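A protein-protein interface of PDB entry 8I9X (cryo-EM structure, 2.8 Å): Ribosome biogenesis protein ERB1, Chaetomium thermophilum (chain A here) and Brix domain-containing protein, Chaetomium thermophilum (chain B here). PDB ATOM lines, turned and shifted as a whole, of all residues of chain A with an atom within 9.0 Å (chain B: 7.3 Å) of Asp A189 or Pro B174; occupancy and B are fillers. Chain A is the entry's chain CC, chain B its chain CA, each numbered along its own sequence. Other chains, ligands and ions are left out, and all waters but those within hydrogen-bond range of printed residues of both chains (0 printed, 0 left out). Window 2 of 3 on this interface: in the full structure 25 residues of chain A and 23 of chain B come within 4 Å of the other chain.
The backbone carbonyl oxygen (O) of Asn A170 sits close to the backbone carbonyl oxygen (O) of Tyr A188, at 2.7 Å.
The side-chain carboxylate (OD1) of Asp A189 lies within hydrogen-bond range of the backbone NH (N) of Gly A192, 3.0 Å away.
The side-chain carboxylate of Asp A189 lies within hydrogen-bond range of the backbone NH of Asn A191.
The backbone carbonyl oxygen (O) of Val A169 lies within hydrogen-bond range of the side-chain hydroxyl (OG1) of Thr A171 (3.1 Å).
OD1 of Asp A189 sits at hydrogen-bond distance from N of Lys A193 (2.7 Å).
OG1 of Thr A171 lies close to O of Tyr A188, 3.4 Å away.
Among the printed residues, merely in contact across the chains: Thr A171 with Ser B172 (3.1 Å), Thr A171 with Lys B173 (3.6 Å), Thr A171 with Pro B174 (3.7 Å), Tyr A188 with Phe B175 (3.6 Å), Asp A189 with Pro B174 (3.2 Å), Ile A190 with Pro B174 (3.1 Å), Gly A192 with Pro B174 (3.6 Å) and Gly A192 with Phe B175 (3.6 Å).
Asp A189 touches just one residue of chain B: Pro B174.
Pro B174 touches just these residues of chain A: Thr A171, Asp A189, Ile A190 and Gly A192.
Printed residues of chain B within 4 Å of Ile A190: Pro B174.
Of the printed residues of chain A, Lys B173 touches Thr A171 (3.6 Å).
Printed residues of chain A within 4 Å of Phe B175: Tyr A188 (3.6 Å) and Gly A192 (3.6 Å).
Ser B136 touches none of the printed residues of chain A.
Pro A168 touches none of the printed residues of chain B.
The nearest residue of chain A that does not touch Pro B174 is Tyr A188 (4.2 Å).
Of the 9 printed residues of chain B, 4 touch a printed residue of chain A.
Printed residues of chain B that touch a printed residue of chain A: Ser B172, Lys B173, Pro B174 and Phe B175.
Hydrophobic or aromatic side chains of chain B that line the printed part of chain A: Pro B174 and Phe B175.
Hydrophobic or aromatic side chains of chain A that line the printed part of chain B: Tyr A188.
Among the printed residues, 8 pairs touch across the chains.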
ATOM      1  N   PRO A 168      32.698  22.964  36.477  1.00  0.00           N
ATOM      2  CA  PRO A 168      32.439  23.586  35.188  1.00  0.00           C
ATOM      3  C   PRO A 168      30.980  23.539  34.719  1.00  0.00           C
ATOM      4  O   PRO A 168      30.277  22.625  35.087  1.00  0.00           O
ATOM      5  CB  PRO A 168      33.268  22.716  34.238  1.00  0.00           C
ATOM      6  CG  PRO A 168      33.529  21.442  34.978  1.00  0.00           C
ATOM      7  CD  PRO A 168      33.705  21.911  36.399  1.00  0.00           C
ATOM      8  N   VAL A 169      30.573  24.495  33.894  1.00  0.00           N
ATOM      9  CA  VAL A 169      29.229  24.488  33.328  1.00  0.00           C
ATOM     10  C   VAL A 169      29.133  23.625  32.075  1.00  0.00           C
ATOM     11  O   VAL A 169      28.035  23.188  31.714  1.00  0.00           O
ATOM     12  CB  VAL A 169      28.796  25.936  33.037  1.00  0.00           C
ATOM     13  CG1 VAL A 169      29.709  26.567  32.004  1.00  0.00           C
ATOM     14  CG2 VAL A 169      27.340  26.008  32.600  1.00  0.00           C
ATOM     15  N   ASN A 170      30.261  23.340  31.421  1.00  0.00           N
ATOM     16  CA  ASN A 170      30.228  22.724  30.097  1.00  0.00           C
ATOM     17  C   ASN A 170      29.614  21.331  30.114  1.00  0.00           C
ATOM     18  O   ASN A 170      29.082  20.886  29.091  1.00  0.00           O
ATOM     19  CB  ASN A 170      31.638  22.662  29.513  1.00  0.00           C
ATOM     20  CG  ASN A 170      31.636  22.447  28.015  1.00  0.00           C
ATOM     21  OD1 ASN A 170      30.602  22.557  27.362  1.00  0.00           O
ATOM     22  ND2 ASN A 170      32.802  22.136  27.460  1.00  0.00           N
ATOM     23  N   THR A 171      29.691  20.624  31.244  1.00  0.00           N
ATOM     24  CA  THR A 171      29.179  19.255  31.363  1.00  0.00           C
ATOM     25  C   THR A 171      29.794  18.368  30.279  1.00  0.00           C
ATOM     26  O   THR A 171      29.175  17.435  29.763  1.00  0.00           O
ATOM     27  CB  THR A 171      27.648  19.232  31.318  1.00  0.00           C
ATOM     28  OG1 THR A 171      27.138  20.236  32.201  1.00  0.00           O
ATOM     29  CG2 THR A 171      27.109  17.895  31.798  1.00  0.00           C
ATOM     30  N   ILE A 172      31.032  18.681  29.919  1.00  0.00           N
ATOM     31  CA  ILE A 172      31.809  17.917  28.954  1.00  0.00           C
ATOM     32  C   ILE A 172      33.002  17.341  29.698  1.00  0.00           C
ATOM     33  O   ILE A 172      33.705  18.068  30.407  1.00  0.00           O
ATOM     34  CB  ILE A 172      32.262  18.795  27.771  1.00  0.00           C
ATOM     35  CG1 ILE A 172      31.064  19.171  26.901  1.00  0.00           C
ATOM     36  CG2 ILE A 172      33.315  18.089  26.945  1.00  0.00           C
ATOM     37  CD1 ILE A 172      30.243  17.992  26.456  1.00  0.00           C
ATOM     38  N   TYR A 180      32.949  19.398  18.023  1.00  0.00           N
ATOM     39  CA  TYR A 180      32.383  20.744  18.065  1.00  0.00           C
ATOM     40  C   TYR A 180      33.174  21.751  17.240  1.00  0.00           C
ATOM     41  O   TYR A 180      32.837  22.940  17.247  1.00  0.00           O
ATOM     42  CB  TYR A 180      32.248  21.276  19.500  1.00  0.00           C
ATOM     43  CG  TYR A 180      31.475  20.401  20.455  1.00  0.00           C
ATOM     44  CD1 TYR A 180      30.101  20.518  20.571  1.00  0.00           C
ATOM     45  CD2 TYR A 180      32.126  19.492  21.275  1.00  0.00           C
ATOM     46  CE1 TYR A 180      29.391  19.735  21.453  1.00  0.00           C
ATOM     47  CE2 TYR A 180      31.423  18.706  22.161  1.00  0.00           C
ATOM     48  CZ  TYR A 180      30.055  18.833  22.248  1.00  0.00           C
ATOM     49  OH  TYR A 180      29.347  18.051  23.128  1.00  0.00           O
ATOM     50  N   HIS A 185      27.981  25.413  18.720  1.00  0.00           N
ATOM     51  CA  HIS A 185      27.868  25.255  20.158  1.00  0.00           C
ATOM     52  C   HIS A 185      29.029  24.426  20.690  1.00  0.00           C
ATOM     53  O   HIS A 185      29.709  23.711  19.950  1.00  0.00           O
ATOM     54  CB  HIS A 185      26.533  24.602  20.529  1.00  0.00           C
ATOM     55  CG  HIS A 185      26.412  23.181  20.076  1.00  0.00           C
ATOM     56  ND1 HIS A 185      26.529  22.113  20.937  1.00  0.00           N
ATOM     57  CD2 HIS A 185      26.188  22.653  18.849  1.00  0.00           C
ATOM     58  CE1 HIS A 185      26.382  20.988  20.262  1.00  0.00           C
ATOM     59  NE2 HIS A 185      26.174  21.287  18.994  1.00  0.00           N
ATOM     60  N   ILE A 186      29.255  24.541  21.995  1.00  0.00           N
ATOM     61  CA  ILE A 186      30.288  23.788  22.698  1.00  0.00           C
ATOM     62  C   ILE A 186      29.650  23.162  23.938  1.00  0.00           C
ATOM     63  O   ILE A 186      29.530  23.803  24.987  1.00  0.00           O
ATOM     64  CB  ILE A 186      31.512  24.654  23.046  1.00  0.00           C
ATOM     65  CG1 ILE A 186      32.635  23.804  23.651  1.00  0.00           C
ATOM     66  CG2 ILE A 186      31.149  25.905  23.868  1.00  0.00           C
ATOM     67  CD1 ILE A 186      33.236  22.808  22.686  1.00  0.00           C
ATOM     68  N   GLY A 187      29.215  21.913  23.812  1.00  0.00           N
ATOM     69  CA  GLY A 187      28.679  21.179  24.939  1.00  0.00           C
ATOM     70  C   GLY A 187      27.240  21.529  25.275  1.00  0.00           C
ATOM     71  O   GLY A 187      26.590  22.362  24.644  1.00  0.00           O
ATOM     72  N   TYR A 188      26.744  20.865  26.317  1.00  0.00           N
ATOM     73  CA  TYR A 188      25.393  21.045  26.832  1.00  0.00           C
ATOM     74  C   TYR A 188      25.467  21.317  28.325  1.00  0.00           C
ATOM     75  O   TYR A 188      26.400  20.871  28.992  1.00  0.00           O
ATOM     76  CB  TYR A 188      24.534  19.803  26.577  1.00  0.00           C
ATOM     77  CG  TYR A 188      23.882  19.768  25.219  1.00  0.00           C
ATOM     78  CD1 TYR A 188      24.624  19.496  24.080  1.00  0.00           C
ATOM     79  CD2 TYR A 188      22.524  19.998  25.076  1.00  0.00           C
ATOM     80  CE1 TYR A 188      24.031  19.460  22.839  1.00  0.00           C
ATOM     81  CE2 TYR A 188      21.923  19.962  23.839  1.00  0.00           C
ATOM     82  CZ  TYR A 188      22.682  19.693  22.724  1.00  0.00           C
ATOM     83  OH  TYR A 188      22.086  19.657  21.486  1.00  0.00           O
ATOM     84  N   ASP A 189      24.488  22.045  28.855  1.00  0.00           N
ATOM     85  CA  ASP A 189      24.482  22.316  30.283  1.00  0.00           C
ATOM     86  C   ASP A 189      23.799  21.178  31.041  1.00  0.00           C
ATOM     87  O   ASP A 189      23.543  20.097  30.504  1.00  0.00           O
ATOM     88  CB  ASP A 189      23.811  23.657  30.584  1.00  0.00           C
ATOM     89  CG  ASP A 189      22.439  23.792  29.954  1.00  0.00           C
ATOM     90  OD1 ASP A 189      21.715  22.780  29.844  1.00  0.00           O
ATOM     91  OD2 ASP A 189      22.078  24.923  29.570  1.00  0.00           O
ATOM     92  N   ILE A 190      23.510  21.431  32.318  1.00  0.00           N
ATOM     93  CA  ILE A 190      22.816  20.462  33.156  1.00  0.00           C
ATOM     94  C   ILE A 190      21.407  20.188  32.654  1.00  0.00           C
ATOM     95  O   ILE A 190      20.967  19.034  32.642  1.00  0.00           O
ATOM     96  CB  ILE A 190      22.774  20.972  34.607  1.00  0.00           C
ATOM     97  CG1 ILE A 190      24.087  20.688  35.322  1.00  0.00           C
ATOM     98  CG2 ILE A 190      21.621  20.344  35.376  1.00  0.00           C
ATOM     99  CD1 ILE A 190      24.241  21.503  36.576  1.00  0.00           C
ATOM    100  N   ASN A 191      20.690  21.227  32.229  1.00  0.00           N
ATOM    101  CA  ASN A 191      19.269  21.104  31.933  1.00  0.00           C
ATOM    102  C   ASN A 191      18.992  20.569  30.537  1.00  0.00           C
ATOM    103  O   ASN A 191      17.822  20.411  30.174  1.00  0.00           O
ATOM    104  CB  ASN A 191      18.588  22.461  32.104  1.00  0.00           C
ATOM    105  CG  ASN A 191      18.767  23.026  33.494  1.00  0.00           C
ATOM    106  OD1 ASN A 191      18.570  22.330  34.488  1.00  0.00           O
ATOM    107  ND2 ASN A 191      19.151  24.294  33.573  1.00  0.00           N
ATOM    108  N   GLY A 192      20.024  20.294  29.749  1.00  0.00           N
ATOM    109  CA  GLY A 192      19.850  19.800  28.400  1.00  0.00           C
ATOM    110  C   GLY A 192      19.880  20.855  27.318  1.00  0.00           C
ATOM    111  O   GLY A 192      19.522  20.552  26.175  1.00  0.00           O
ATOM    112  N   LYS A 193      20.291  22.077  27.637  1.00  0.00           N
ATOM    113  CA  LYS A 193      20.371  23.164  26.676  1.00  0.00           C
ATOM    114  C   LYS A 193      21.818  23.343  26.241  1.00  0.00           C
ATOM    115  O   LYS A 193      22.727  23.356  27.075  1.00  0.00           O
ATOM    116  CB  LYS A 193      19.834  24.464  27.277  1.00  0.00           C
ATOM    117  CG  LYS A 193      18.382  24.387  27.716  1.00  0.00           C
ATOM    118  CD  LYS A 193      17.455  24.190  26.532  1.00  0.00           C
ATOM    119  CE  LYS A 193      16.000  24.283  26.951  1.00  0.00           C
ATOM    120  NZ  LYS A 193      15.591  23.128  27.798  1.00  0.00           N
ATOM    121  N   LYS A 194      22.032  23.470  24.936  1.00  0.00           N
ATOM    122  CA  LYS A 194      23.392  23.545  24.424  1.00  0.00           C
ATOM    123  C   LYS A 194      24.013  24.902  24.730  1.00  0.00           C
ATOM    124  O   LYS A 194      23.311  25.903  24.899  1.00  0.00           O
ATOM    125  CB  LYS A 194      23.412  23.268  22.921  1.00  0.00           C
ATOM    126  CG  LYS A 194      22.689  24.291  22.075  1.00  0.00           C
ATOM    127  CD  LYS A 194      22.791  23.929  20.603  1.00  0.00           C
ATOM    128  CE  LYS A 194      21.913  22.738  20.267  1.00  0.00           C
ATOM    129  NZ  LYS A 194      21.900  22.453  18.808  1.00  0.00           N
ATOM    130  N   ILE A 195      25.340  24.926  24.810  1.00  0.00           N
ATOM    131  CA  ILE A 195      26.084  26.134  25.147  1.00  0.00           C
ATOM    132  C   ILE A 195      26.670  26.710  23.866  1.00  0.00           C
ATOM    133  O   ILE A 195      27.511  26.077  23.220  1.00  0.00           O
ATOM    134  CB  ILE A 195      27.189  25.840  26.172  1.00  0.00           C
ATOM    135  CG1 ILE A 195      26.587  25.301  27.469  1.00  0.00           C
ATOM    136  CG2 ILE A 195      28.003  27.089  26.442  1.00  0.00           C
ATOM    137  CD1 ILE A 195      27.595  24.645  28.374  1.00  0.00           C
ATOM    138  N   MET A 196      26.241  27.915  23.512  1.00  0.00           N
ATOM    139  CA  MET A 196      26.625  28.514  22.246  1.00  0.00           C
ATOM    140  C   MET A 196      27.975  29.213  22.368  1.00  0.00           C
ATOM    141  O   MET A 196      28.312  29.797  23.402  1.00  0.00           O
ATOM    142  CB  MET A 196      25.557  29.503  21.782  1.00  0.00           C
ATOM    143  CG  MET A 196      24.142  28.937  21.782  1.00  0.00           C
ATOM    144  SD  MET A 196      23.808  27.620  20.593  1.00  0.00           S
ATOM    145  CE  MET A 196      24.891  28.054  19.236  1.00  0.00           C
ATOM    146  N   LEU B 133      26.823   7.513  29.165  1.00  0.00           N
ATOM    147  CA  LEU B 133      27.410   8.806  29.585  1.00  0.00           C
ATOM    148  C   LEU B 133      27.864   8.720  31.043  1.00  0.00           C
ATOM    149  O   LEU B 133      27.053   8.318  31.878  1.00  0.00           O
ATOM    150  CB  LEU B 133      26.333   9.873  29.410  1.00  0.00           C
ATOM    151  CG  LEU B 133      26.153  10.458  28.016  1.00  0.00           C
ATOM    152  CD1 LEU B 133      24.742  10.988  27.846  1.00  0.00           C
ATOM    153  CD2 LEU B 133      27.158  11.564  27.775  1.00  0.00           C
ATOM    154  N   GLY B 135      28.130   9.864  34.506  1.00  0.00           N
ATOM    155  CA  GLY B 135      27.530  10.910  35.341  1.00  0.00           C
ATOM    156  C   GLY B 135      26.077  11.102  35.005  1.00  0.00           C
ATOM    157  O   GLY B 135      25.388  11.798  35.755  1.00  0.00           O
ATOM    158  N   SER B 136      25.632  10.513  33.907  1.00  0.00           N
ATOM    159  CA  SER B 136      24.203  10.581  33.546  1.00  0.00           C
ATOM    160  C   SER B 136      23.413   9.952  34.666  1.00  0.00           C
ATOM    161  O   SER B 136      23.885   9.001  35.273  1.00  0.00           O
ATOM    162  CB  SER B 136      23.913   9.938  32.218  1.00  0.00           C
ATOM    163  OG  SER B 136      24.352   8.594  32.194  1.00  0.00           O
ATOM    164  N   ARG B 137      22.231  10.471  34.890  1.00  0.00           N
ATOM    165  CA  ARG B 137      21.398   9.996  36.003  1.00  0.00           C
ATOM    166  C   ARG B 137      20.728   8.708  35.588  1.00  0.00           C
ATOM    167  O   ARG B 137      20.082   8.681  34.544  1.00  0.00           O
ATOM    168  CB  ARG B 137      20.372  11.069  36.329  1.00  0.00           C
ATOM    169  CG  ARG B 137      20.929  12.442  36.660  1.00  0.00           C
ATOM    170  CD  ARG B 137      19.802  13.242  37.276  1.00  0.00           C
ATOM    171  NE  ARG B 137      19.262  12.527  38.421  1.00  0.00           N
ATOM    172  CZ  ARG B 137      17.995  12.554  38.806  1.00  0.00           C
ATOM    173  NH1 ARG B 137      17.113  13.260  38.126  1.00  0.00           N
ATOM    174  NH2 ARG B 137      17.612  11.870  39.867  1.00  0.00           N
ATOM    175  N   SER B 172      26.838  16.083  36.981  1.00  0.00           N
ATOM    176  CA  SER B 172      26.041  15.095  36.221  1.00  0.00           C
ATOM    177  C   SER B 172      25.906  15.462  34.746  1.00  0.00           C
ATOM    178  O   SER B 172      26.104  16.641  34.440  1.00  0.00           O
ATOM    179  CB  SER B 172      24.689  15.026  36.835  1.00  0.00           C
ATOM    180  OG  SER B 172      23.913  16.161  36.490  1.00  0.00           O
ATOM    181  N   LYS B 173      25.563  14.511  33.874  1.00  0.00           N
ATOM    182  CA  LYS B 173      25.244  14.771  32.479  1.00  0.00           C
ATOM    183  C   LYS B 173      23.739  14.983  32.310  1.00  0.00           C
ATOM    184  O   LYS B 173      22.943  14.482  33.109  1.00  0.00           O
ATOM    185  CB  LYS B 173      25.712  13.614  31.603  1.00  0.00           C
ATOM    186  CG  LYS B 173      27.180  13.276  31.759  1.00  0.00           C
ATOM    187  CD  LYS B 173      28.062  14.355  31.169  1.00  0.00           C
ATOM    188  CE  LYS B 173      29.525  14.099  31.477  1.00  0.00           C
ATOM    189  NZ  LYS B 173      30.036  12.903  30.760  1.00  0.00           N
ATOM    190  N   PRO B 174      23.320  15.718  31.274  1.00  0.00           N
ATOM    191  CA  PRO B 174      21.905  16.099  31.162  1.00  0.00           C
ATOM    192  C   PRO B 174      20.979  15.026  30.608  1.00  0.00           C
ATOM    193  O   PRO B 174      19.808  14.988  31.013  1.00  0.00           O
ATOM    194  CB  PRO B 174      21.953  17.305  30.221  1.00  0.00           C
ATOM    195  CG  PRO B 174      23.118  17.044  29.362  1.00  0.00           C
ATOM    196  CD  PRO B 174      24.138  16.357  30.229  1.00  0.00           C
ATOM    197  N   PHE B 175      21.441  14.165  29.708  1.00  0.00           N
ATOM    198  CA  PHE B 175      20.576  13.196  29.050  1.00  0.00           C
ATOM    199  C   PHE B 175      20.815  11.813  29.635  1.00  0.00           C
ATOM    200  O   PHE B 175      21.956  11.416  29.889  1.00  0.00           O
ATOM    201  CB  PHE B 175      20.811  13.187  27.534  1.00  0.00           C
ATOM    202  CG  PHE B 175      20.700  14.543  26.905  1.00  0.00           C
ATOM    203  CD1 PHE B 175      19.465  15.092  26.620  1.00  0.00           C
ATOM    204  CD2 PHE B 175      21.834  15.285  26.627  1.00  0.00           C
ATOM    205  CE1 PHE B 175      19.362  16.342  26.051  1.00  0.00           C
ATOM    206  CE2 PHE B 175      21.737  16.539  26.064  1.00  0.00           C
ATOM    207  CZ  PHE B 175      20.499  17.068  25.775  1.00  0.00           C
ATOM    208  N   ILE B 176      19.727  11.083  29.855  1.00  0.00           N
ATOM    209  CA  ILE B 176      19.766   9.811  30.567  1.00  0.00           C
ATOM    210  C   ILE B 176      19.683   8.674  29.558  1.00  0.00           C
ATOM    211  O   ILE B 176      18.832   8.684  28.660  1.00  0.00           O
ATOM    212  CB  ILE B 176      18.643   9.724  31.614  1.00  0.00           C
ATOM    213  CG1 ILE B 176      17.271   9.794  30.957  1.00  0.00           C
ATOM    214  CG2 ILE B 176      18.772  10.858  32.618  1.00  0.00           C
ATOM    215  CD1 ILE B 176      16.164   9.478  31.899  1.00  0.00           C
